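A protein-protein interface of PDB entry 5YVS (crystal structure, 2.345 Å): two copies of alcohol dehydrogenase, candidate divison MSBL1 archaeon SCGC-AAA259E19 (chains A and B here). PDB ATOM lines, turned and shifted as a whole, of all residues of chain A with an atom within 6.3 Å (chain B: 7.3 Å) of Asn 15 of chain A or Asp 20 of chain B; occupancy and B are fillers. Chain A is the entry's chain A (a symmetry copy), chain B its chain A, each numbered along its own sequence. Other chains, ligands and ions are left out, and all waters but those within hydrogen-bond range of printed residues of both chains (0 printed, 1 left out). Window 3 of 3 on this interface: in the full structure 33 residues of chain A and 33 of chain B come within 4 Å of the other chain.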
ATOM      1  N   ARG A  13       8.610  32.175   7.881  1.00  0.00           N
ATOM      2  CA  ARG A  13       8.872  31.214   8.944  1.00  0.00           C
ATOM      3  C   ARG A  13       9.521  29.985   8.326  1.00  0.00           C
ATOM      4  O   ARG A  13       8.970  29.389   7.393  1.00  0.00           O
ATOM      5  CB  ARG A  13       7.589  30.842   9.689  1.00  0.00           C
ATOM      6  CG  ARG A  13       7.822  29.899  10.859  1.00  0.00           C
ATOM      7  CD  ARG A  13       6.654  29.905  11.830  1.00  0.00           C
ATOM      8  NE  ARG A  13       6.983  29.208  13.070  1.00  0.00           N
ATOM      9  CZ  ARG A  13       6.259  29.282  14.183  1.00  0.00           C
ATOM     10  NH1 ARG A  13       5.162  30.029  14.218  1.00  0.00           N
ATOM     11  NH2 ARG A  13       6.637  28.612  15.263  1.00  0.00           N
ATOM     12  N   HIS A  14      10.695  29.621   8.837  1.00  0.00           N
ATOM     13  CA  HIS A  14      11.464  28.480   8.358  1.00  0.00           C
ATOM     14  C   HIS A  14      11.242  27.291   9.285  1.00  0.00           C
ATOM     15  O   HIS A  14      11.459  27.397  10.497  1.00  0.00           O
ATOM     16  CB  HIS A  14      12.952  28.842   8.287  1.00  0.00           C
ATOM     17  CG  HIS A  14      13.878  27.663   8.323  1.00  0.00           C
ATOM     18  ND1 HIS A  14      14.547  27.209   7.207  1.00  0.00           N
ATOM     19  CD2 HIS A  14      14.266  26.861   9.344  1.00  0.00           C
ATOM     20  CE1 HIS A  14      15.297  26.172   7.534  1.00  0.00           C
ATOM     21  NE2 HIS A  14      15.142  25.938   8.825  1.00  0.00           N
ATOM     22  N   ASN A  15      10.815  26.164   8.714  1.00  0.00           N
ATOM     23  CA  ASN A  15      10.612  24.924   9.460  1.00  0.00           C
ATOM     24  C   ASN A  15      11.289  23.777   8.727  1.00  0.00           C
ATOM     25  O   ASN A  15      10.937  23.471   7.582  1.00  0.00           O
ATOM     26  CB  ASN A  15       9.124  24.622   9.648  1.00  0.00           C
ATOM     27  CG  ASN A  15       8.464  25.558  10.627  1.00  0.00           C
ATOM     28  OD1 ASN A  15       7.789  26.507  10.234  1.00  0.00           O
ATOM     29  ND2 ASN A  15       8.658  25.298  11.916  1.00  0.00           N
ATOM     30  N   LEU A  16      12.244  23.140   9.390  1.00  0.00           N
ATOM     31  CA  LEU A  16      12.951  21.997   8.833  1.00  0.00           C
ATOM     32  C   LEU A  16      13.200  20.979   9.935  1.00  0.00           C
ATOM     33  O   LEU A  16      13.914  21.276  10.900  1.00  0.00           O
ATOM     34  CB  LEU A  16      14.272  22.437   8.201  1.00  0.00           C
ATOM     35  CG  LEU A  16      15.135  21.337   7.587  1.00  0.00           C
ATOM     36  CD1 LEU A  16      14.415  20.697   6.416  1.00  0.00           C
ATOM     37  CD2 LEU A  16      16.481  21.897   7.153  1.00  0.00           C
ATOM     38  N   PRO A  17      12.629  19.780   9.841  1.00  0.00           N
ATOM     39  CA  PRO A  17      12.851  18.779  10.890  1.00  0.00           C
ATOM     40  C   PRO A  17      14.305  18.334  10.930  1.00  0.00           C
ATOM     41  O   PRO A  17      15.066  18.520   9.980  1.00  0.00           O
ATOM     42  CB  PRO A  17      11.923  17.625  10.487  1.00  0.00           C
ATOM     43  CG  PRO A  17      10.909  18.246   9.562  1.00  0.00           C
ATOM     44  CD  PRO A  17      11.655  19.326   8.836  1.00  0.00           C
ATOM     45  N   THR A 230      16.082  30.679   3.112  1.00  0.00           N
ATOM     46  CA  THR A 230      16.872  29.559   3.605  1.00  0.00           C
ATOM     47  C   THR A 230      16.933  28.405   2.611  1.00  0.00           C
ATOM     48  O   THR A 230      17.873  27.605   2.667  1.00  0.00           O
ATOM     49  CB  THR A 230      16.319  29.069   4.945  1.00  0.00           C
ATOM     50  OG1 THR A 230      14.944  28.704   4.793  1.00  0.00           O
ATOM     51  CG2 THR A 230      16.422  30.168   5.982  1.00  0.00           C
ATOM     52  N   THR A 274      11.158  20.854   1.493  1.00  0.00           N
ATOM     53  CA  THR A 274      10.594  20.892   2.838  1.00  0.00           C
ATOM     54  C   THR A 274      10.385  22.329   3.299  1.00  0.00           C
ATOM     55  O   THR A 274       9.296  22.693   3.758  1.00  0.00           O
ATOM     56  CB  THR A 274      11.510  20.146   3.813  1.00  0.00           C
ATOM     57  OG1 THR A 274      11.677  18.793   3.376  1.00  0.00           O
ATOM     58  CG2 THR A 274      10.920  20.147   5.217  1.00  0.00           C
ATOM     59  N   ILE A 275      11.425  23.160   3.174  1.00  0.00           N
ATOM     60  CA  ILE A 275      11.357  24.545   3.631  1.00  0.00           C
ATOM     61  C   ILE A 275      10.340  25.334   2.816  1.00  0.00           C
ATOM     62  O   ILE A 275       9.497  26.050   3.368  1.00  0.00           O
ATOM     63  CB  ILE A 275      12.751  25.195   3.558  1.00  0.00           C
ATOM     64  CG1 ILE A 275      13.726  24.485   4.501  1.00  0.00           C
ATOM     65  CG2 ILE A 275      12.662  26.681   3.869  1.00  0.00           C
ATOM     66  CD1 ILE A 275      15.178  24.800   4.214  1.00  0.00           C
ATOM     67  N   PRO B  17      20.003  19.683  13.666  1.00  0.00           N
ATOM     68  CA  PRO B  17      18.798  19.510  14.484  1.00  0.00           C
ATOM     69  C   PRO B  17      17.625  20.290  13.910  1.00  0.00           C
ATOM     70  O   PRO B  17      17.788  21.208  13.106  1.00  0.00           O
ATOM     71  CB  PRO B  17      19.214  20.053  15.857  1.00  0.00           C
ATOM     72  CG  PRO B  17      20.721  20.019  15.849  1.00  0.00           C
ATOM     73  CD  PRO B  17      21.107  20.292  14.424  1.00  0.00           C
ATOM     74  N   SER B  18      16.423  19.904  14.333  1.00  0.00           N
ATOM     75  CA  SER B  18      15.220  20.615  13.922  1.00  0.00           C
ATOM     76  C   SER B  18      15.381  22.112  14.150  1.00  0.00           C
ATOM     77  O   SER B  18      15.915  22.545  15.173  1.00  0.00           O
ATOM     78  CB  SER B  18      14.009  20.097  14.701  1.00  0.00           C
ATOM     79  OG  SER B  18      12.948  21.038  14.666  1.00  0.00           O
ATOM     80  N   SER B  19      14.916  22.905  13.188  1.00  0.00           N
ATOM     81  CA  SER B  19      15.017  24.356  13.261  1.00  0.00           C
ATOM     82  C   SER B  19      13.660  24.995  12.996  1.00  0.00           C
ATOM     83  O   SER B  19      12.929  24.573  12.094  1.00  0.00           O
ATOM     84  CB  SER B  19      16.057  24.893  12.265  1.00  0.00           C
ATOM     85  OG  SER B  19      15.790  24.446  10.949  1.00  0.00           O
ATOM     86  N   ASP B  20      13.337  26.015  13.792  1.00  0.00           N
ATOM     87  CA  ASP B  20      12.076  26.756  13.683  1.00  0.00           C
ATOM     88  C   ASP B  20      12.422  28.239  13.783  1.00  0.00           C
ATOM     89  O   ASP B  20      12.708  28.740  14.873  1.00  0.00           O
ATOM     90  CB  ASP B  20      11.096  26.331  14.774  1.00  0.00           C
ATOM     91  CG  ASP B  20       9.723  26.961  14.612  1.00  0.00           C
ATOM     92  OD1 ASP B  20       9.534  27.769  13.681  1.00  0.00           O
ATOM     93  OD2 ASP B  20       8.826  26.640  15.422  1.00  0.00           O
ATOM     94  N   ILE B  21      12.402  28.939  12.649  1.00  0.00           N
ATOM     95  CA  ILE B  21      12.877  30.318  12.567  1.00  0.00           C
ATOM     96  C   ILE B  21      11.699  31.220  12.220  1.00  0.00           C
ATOM     97  O   ILE B  21      11.037  31.021  11.194  1.00  0.00           O
ATOM     98  CB  ILE B  21      14.006  30.465  11.534  1.00  0.00           C
ATOM     99  CG1 ILE B  21      15.128  29.468  11.827  1.00  0.00           C
ATOM    100  CG2 ILE B  21      14.547  31.885  11.539  1.00  0.00           C
ATOM    101  CD1 ILE B  21      16.245  29.473  10.810  1.00  0.00           C
ATOM    102  N   ILE B  22      11.446  32.212  13.070  1.00  0.00           N
ATOM    103  CA  ILE B  22      10.440  33.239  12.818  1.00  0.00           C
ATOM    104  C   ILE B  22      11.183  34.514  12.447  1.00  0.00           C
ATOM    105  O   ILE B  22      11.887  35.099  13.277  1.00  0.00           O
ATOM    106  CB  ILE B  22       9.531  33.465  14.029  1.00  0.00           C
ATOM    107  CG1 ILE B  22       8.934  32.142  14.508  1.00  0.00           C
ATOM    108  CG2 ILE B  22       8.433  34.455  13.677  1.00  0.00           C
ATOM    109  CD1 ILE B  22       8.123  32.262  15.784  1.00  0.00           C
ATOM    110  N   GLU B  34       5.130  31.235  21.611  1.00  0.00           N
ATOM    111  CA  GLU B  34       6.038  30.128  21.332  1.00  0.00           C
ATOM    112  C   GLU B  34       6.606  29.538  22.616  1.00  0.00           C
ATOM    113  O   GLU B  34       6.699  28.313  22.755  1.00  0.00           O
ATOM    114  CB  GLU B  34       7.159  30.598  20.407  1.00  0.00           C
ATOM    115  CG  GLU B  34       6.675  31.078  19.048  1.00  0.00           C
ATOM    116  CD  GLU B  34       5.982  29.983  18.263  1.00  0.00           C
ATOM    117  OE1 GLU B  34       4.986  30.278  17.567  1.00  0.00           O
ATOM    118  OE2 GLU B  34       6.433  28.823  18.344  1.00  0.00           O
ATOM    119  N   LYS B  37       4.405  26.950  24.502  1.00  0.00           N
ATOM    120  CA  LYS B  37       4.398  25.579  24.007  1.00  0.00           C
ATOM    121  C   LYS B  37       5.427  24.705  24.708  1.00  0.00           C
ATOM    122  O   LYS B  37       5.340  23.474  24.628  1.00  0.00           O
ATOM    123  CB  LYS B  37       4.659  25.559  22.497  1.00  0.00           C
ATOM    124  CG  LYS B  37       3.639  26.311  21.657  1.00  0.00           C
ATOM    125  CD  LYS B  37       4.044  26.295  20.191  1.00  0.00           C
ATOM    126  CE  LYS B  37       3.064  27.071  19.325  1.00  0.00           C
ATOM    127  NZ  LYS B  37       3.525  27.155  17.911  1.00  0.00           N
ATOM    128  N   TRP B  38       6.395  25.312  25.398  1.00  0.00           N
ATOM    129  CA  TRP B  38       7.501  24.582  25.995  1.00  0.00           C
ATOM    130  C   TRP B  38       7.587  24.696  27.508  1.00  0.00           C
ATOM    131  O   TRP B  38       8.271  23.873  28.127  1.00  0.00           O
ATOM    132  CB  TRP B  38       8.831  25.050  25.387  1.00  0.00           C
ATOM    133  CG  TRP B  38       8.908  24.722  23.944  1.00  0.00           C
ATOM    134  CD1 TRP B  38       8.555  25.522  22.900  1.00  0.00           C
ATOM    135  CD2 TRP B  38       9.332  23.481  23.379  1.00  0.00           C
ATOM    136  NE1 TRP B  38       8.748  24.858  21.713  1.00  0.00           N
ATOM    137  CE2 TRP B  38       9.226  23.601  21.981  1.00  0.00           C
ATOM    138  CE3 TRP B  38       9.798  22.280  23.920  1.00  0.00           C
ATOM    139  CZ2 TRP B  38       9.570  22.566  21.115  1.00  0.00           C
ATOM    140  CZ3 TRP B  38      10.138  21.254  23.060  1.00  0.00           C
ATOM    141  CH2 TRP B  38      10.024  21.403  21.673  1.00  0.00           C
ATOM    142  N   ALA B 154      15.215  31.402  21.654  1.00  0.00           N
ATOM    143  CA  ALA B 154      16.265  32.370  21.356  1.00  0.00           C
ATOM    144  C   ALA B 154      15.717  33.486  20.477  1.00  0.00           C
ATOM    145  O   ALA B 154      15.238  33.231  19.367  1.00  0.00           O
ATOM    146  CB  ALA B 154      17.454  31.693  20.674  1.00  0.00           C
ATOM    147  N   HIS B 164      21.370  31.738  17.478  1.00  0.00           N
ATOM    148  CA  HIS B 164      19.961  31.373  17.534  1.00  0.00           C
ATOM    149  C   HIS B 164      19.664  30.107  16.743  1.00  0.00           C
ATOM    150  O   HIS B 164      18.601  29.510  16.939  1.00  0.00           O
ATOM    151  CB  HIS B 164      19.091  32.531  17.035  1.00  0.00           C
ATOM    152  CG  HIS B 164      19.365  32.931  15.617  1.00  0.00           C
ATOM    153  ND1 HIS B 164      20.542  33.534  15.228  1.00  0.00           N
ATOM    154  CD2 HIS B 164      18.610  32.825  14.498  1.00  0.00           C
ATOM    155  CE1 HIS B 164      20.503  33.775  13.929  1.00  0.00           C
ATOM    156  NE2 HIS B 164      19.342  33.354  13.462  1.00  0.00           N
ATOM    157  N   VAL B 165      20.571  29.682  15.861  1.00  0.00           N
ATOM    158  CA  VAL B 165      20.389  28.437  15.120  1.00  0.00           C
ATOM    159  C   VAL B 165      21.683  27.629  15.127  1.00  0.00           C
ATOM    160  O   VAL B 165      22.100  27.097  14.092  1.00  0.00           O
ATOM    161  CB  VAL B 165      19.905  28.700  13.681  1.00  0.00           C
ATOM    162  CG1 VAL B 165      18.438  29.102  13.685  1.00  0.00           C
ATOM    163  CG2 VAL B 165      20.763  29.770  13.000  1.00  0.00           C
ATOM    164  N   PHE B 188      20.096  22.926  20.960  1.00  0.00           N
ATOM    165  CA  PHE B 188      19.667  23.756  19.835  1.00  0.00           C
ATOM    166  C   PHE B 188      18.329  24.407  20.168  1.00  0.00           C
ATOM    167  O   PHE B 188      17.394  23.710  20.578  1.00  0.00           O
ATOM    168  CB  PHE B 188      19.545  22.909  18.565  1.00  0.00           C
ATOM    169  CG  PHE B 188      19.509  23.709  17.279  1.00  0.00           C
ATOM    170  CD1 PHE B 188      18.344  24.340  16.866  1.00  0.00           C
ATOM    171  CD2 PHE B 188      20.633  23.800  16.470  1.00  0.00           C
ATOM    172  CE1 PHE B 188      18.308  25.061  15.682  1.00  0.00           C
ATOM    173  CE2 PHE B 188      20.602  24.521  15.282  1.00  0.00           C
ATOM    174  CZ  PHE B 188      19.437  25.150  14.889  1.00  0.00           C
ATOM    175  N   PRO B 189      18.199  25.724  20.015  1.00  0.00           N
ATOM    176  CA  PRO B 189      16.944  26.395  20.378  1.00  0.00           C
ATOM    177  C   PRO B 189      15.735  25.758  19.702  1.00  0.00           C
ATOM    178  O   PRO B 189      15.766  25.418  18.519  1.00  0.00           O
ATOM    179  CB  PRO B 189      17.167  27.833  19.898  1.00  0.00           C
ATOM    180  CG  PRO B 189      18.647  28.011  19.952  1.00  0.00           C
ATOM    181  CD  PRO B 189      19.220  26.679  19.552  1.00  0.00           C
ATOM    182  N   LYS B 190      14.658  25.591  20.476  1.00  0.00           N
ATOM    183  CA  LYS B 190      13.430  25.048  19.904  1.00  0.00           C
ATOM    184  C   LYS B 190      12.808  26.027  18.916  1.00  0.00           C
ATOM    185  O   LYS B 190      12.319  25.622  17.854  1.00  0.00           O
ATOM    186  CB  LYS B 190      12.428  24.701  21.008  1.00  0.00           C
ATOM    187  CG  LYS B 190      12.990  23.861  22.144  1.00  0.00           C
ATOM    188  CD  LYS B 190      13.501  22.516  21.659  1.00  0.00           C
ATOM    189  CE  LYS B 190      14.039  21.689  22.814  1.00  0.00           C
ATOM    190  NZ  LYS B 190      14.610  20.402  22.339  1.00  0.00           N
ATOM    191  N   VAL B 191      12.813  27.315  19.250  1.00  0.00           N
ATOM    192  CA  VAL B 191      12.278  28.359  18.386  1.00  0.00           C
ATOM    193  C   VAL B 191      13.281  29.499  18.330  1.00  0.00           C
ATOM    194  O   VAL B 191      13.875  29.869  19.349  1.00  0.00           O
ATOM    195  CB  VAL B 191      10.906  28.868  18.874  1.00  0.00           C
ATOM    196  CG1 VAL B 191      10.386  29.950  17.940  1.00  0.00           C
ATOM    197  CG2 VAL B 191       9.920  27.718  18.970  1.00  0.00           C
ATOM    198  N   SER B 192      13.469  30.055  17.137  1.00  0.00           N
ATOM    199  CA  SER B 192      14.414  31.138  16.904  1.00  0.00           C
ATOM    200  C   SER B 192      13.665  32.329  16.325  1.00  0.00           C
ATOM    201  O   SER B 192      12.963  32.195  15.317  1.00  0.00           O
ATOM    202  CB  SER B 192      15.529  30.693  15.956  1.00  0.00           C
ATOM    203  OG  SER B 192      16.114  29.481  16.397  1.00  0.00           O
ATOM    204  N   ILE B 193      13.814  33.489  16.959  1.00  0.00           N
ATOM    205  CA  ILE B 193      13.116  34.702  16.551  1.00  0.00           C
ATOM    206  C   ILE B 193      14.146  35.727  16.100  1.00  0.00           C
ATOM    207  O   ILE B 193      15.042  36.098  16.868  1.00  0.00           O
ATOM    208  CB  ILE B 193      12.246  35.271  17.680  1.00  0.00           C
ATOM    209  CG1 ILE B 193      11.161  34.262  18.065  1.00  0.00           C
ATOM    210  CG2 ILE B 193      11.633  36.595  17.254  1.00  0.00           C
ATOM    211  CD1 ILE B 193      10.376  34.641  19.304  1.00  0.00           C
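Printed residues of chain A that touch a printed residue of chain B: Arg 13, His 14, Asn 15, Leu 16 and Pro 17.
Of the 18 printed residues of chain B, 6 touch a printed residue of chain A.
Among the printed residues, Asp or Glu carboxylates within 4 Å of a Lys or Arg side-chain nitrogen of the other chain: Arg 13 of chain A with Asp 20 of chain B and Arg 13 of chain A with Glu 34 of chain B.
Among the printed residues, merely in contact across the chains: Arg 13 of chain A with Ile 21 of chain B (3.1 Å), His 14 of chain A with Asp 20 of chain B (3.3 Å), Leu 16 of chain A with Ser 18 of chain B (3.4 Å), Asn 15 of chain A with Ser 19 of chain B (3.5 Å), Arg 13 of chain A with Ile 22 of chain B (3.8 Å) and Pro 17 of chain A with Ser 18 of chain B (3.9 Å).
1 position is printed for both chains.
Of the 12 pairs that touch across the chains among the printed residues, none has its exchanged pair printed and touching as well.
OG of Ser 19 of chain B is in hydrogen-bond range of NE2 of His 14 of chain A (2.7 Å).
The backbone carbonyl oxygen (O) of Leu 16 of chain A lies within hydrogen-bond range of the backbone NH (N) of Ser 19 of chain B (3.0 Å).
NH2 of Arg 13 of chain A lies within salt-bridge range of OD2 of Asp 20 of chain B (3.0 Å).
The side-chain carboxylate (OD1) of Asp 20 of chain B sits at hydrogen-bond distance from the side-chain amide nitrogen (ND2) of Asn 15 of chain A (3.2 Å).
The backbone carbonyl oxygen (O) of Ile 21 of chain B is in hydrogen-bond range of the backbone NH (N) of His 14 of chain A (2.8 Å).
NH2 of Arg 13 of chain A is in salt-bridge range of OE2 of Glu 34 of chain B, at 3.1 Å.
The backbone NH of Ser 192 of chain B lies within hydrogen-bond range of the backbone carbonyl oxygen of Asp 20 of chain B, at 2.7 Å.
The backbone NH of Ile 22 of chain B lies within hydrogen-bond range of the backbone carbonyl oxygen of Ser 192 of chain B, 2.7 Å away.
The side-chain carboxylate of Glu 34 of chain B lies within salt-bridge range of the side-chain amino group of Lys 37 of chain B (3.4 Å).
The side-chain hydroxyl of Thr 230 of chain A is in hydrogen-bond range of a ring nitrogen (ND1) of His 14 of chain A (2.9 Å).
Printed residues of chain B within 4 Å of Arg 13 of chain A: Asp 20 (3.0 Å), Ile 21 (3.1 Å), Ile 22 (3.8 Å) and Glu 34 (3.1 Å).
Asn 15 of chain A touches two residues of chain B.
Printed residues of chain B within 4 Å of Leu 16 of chain A: Ser 18 (3.4 Å) and Ser 19 (3.0 Å).
Of the printed residues of chain A, Ser 19 of chain B touches His 14 (2.7 Å), Asn 15 (3.5 Å) and Leu 16 (3.0 Å).
Printed residues of chain A within 4 Å of Ile 21 of chain B: Arg 13 (3.1 Å) and His 14 (2.8 Å).
Of the printed residues of chain A, Glu 34 of chain B touches Arg 13 (3.1 Å).
The nearest residue of chain B that does not touch Asn 15 of chain A is Ile 21 of chain B (5.1 Å).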
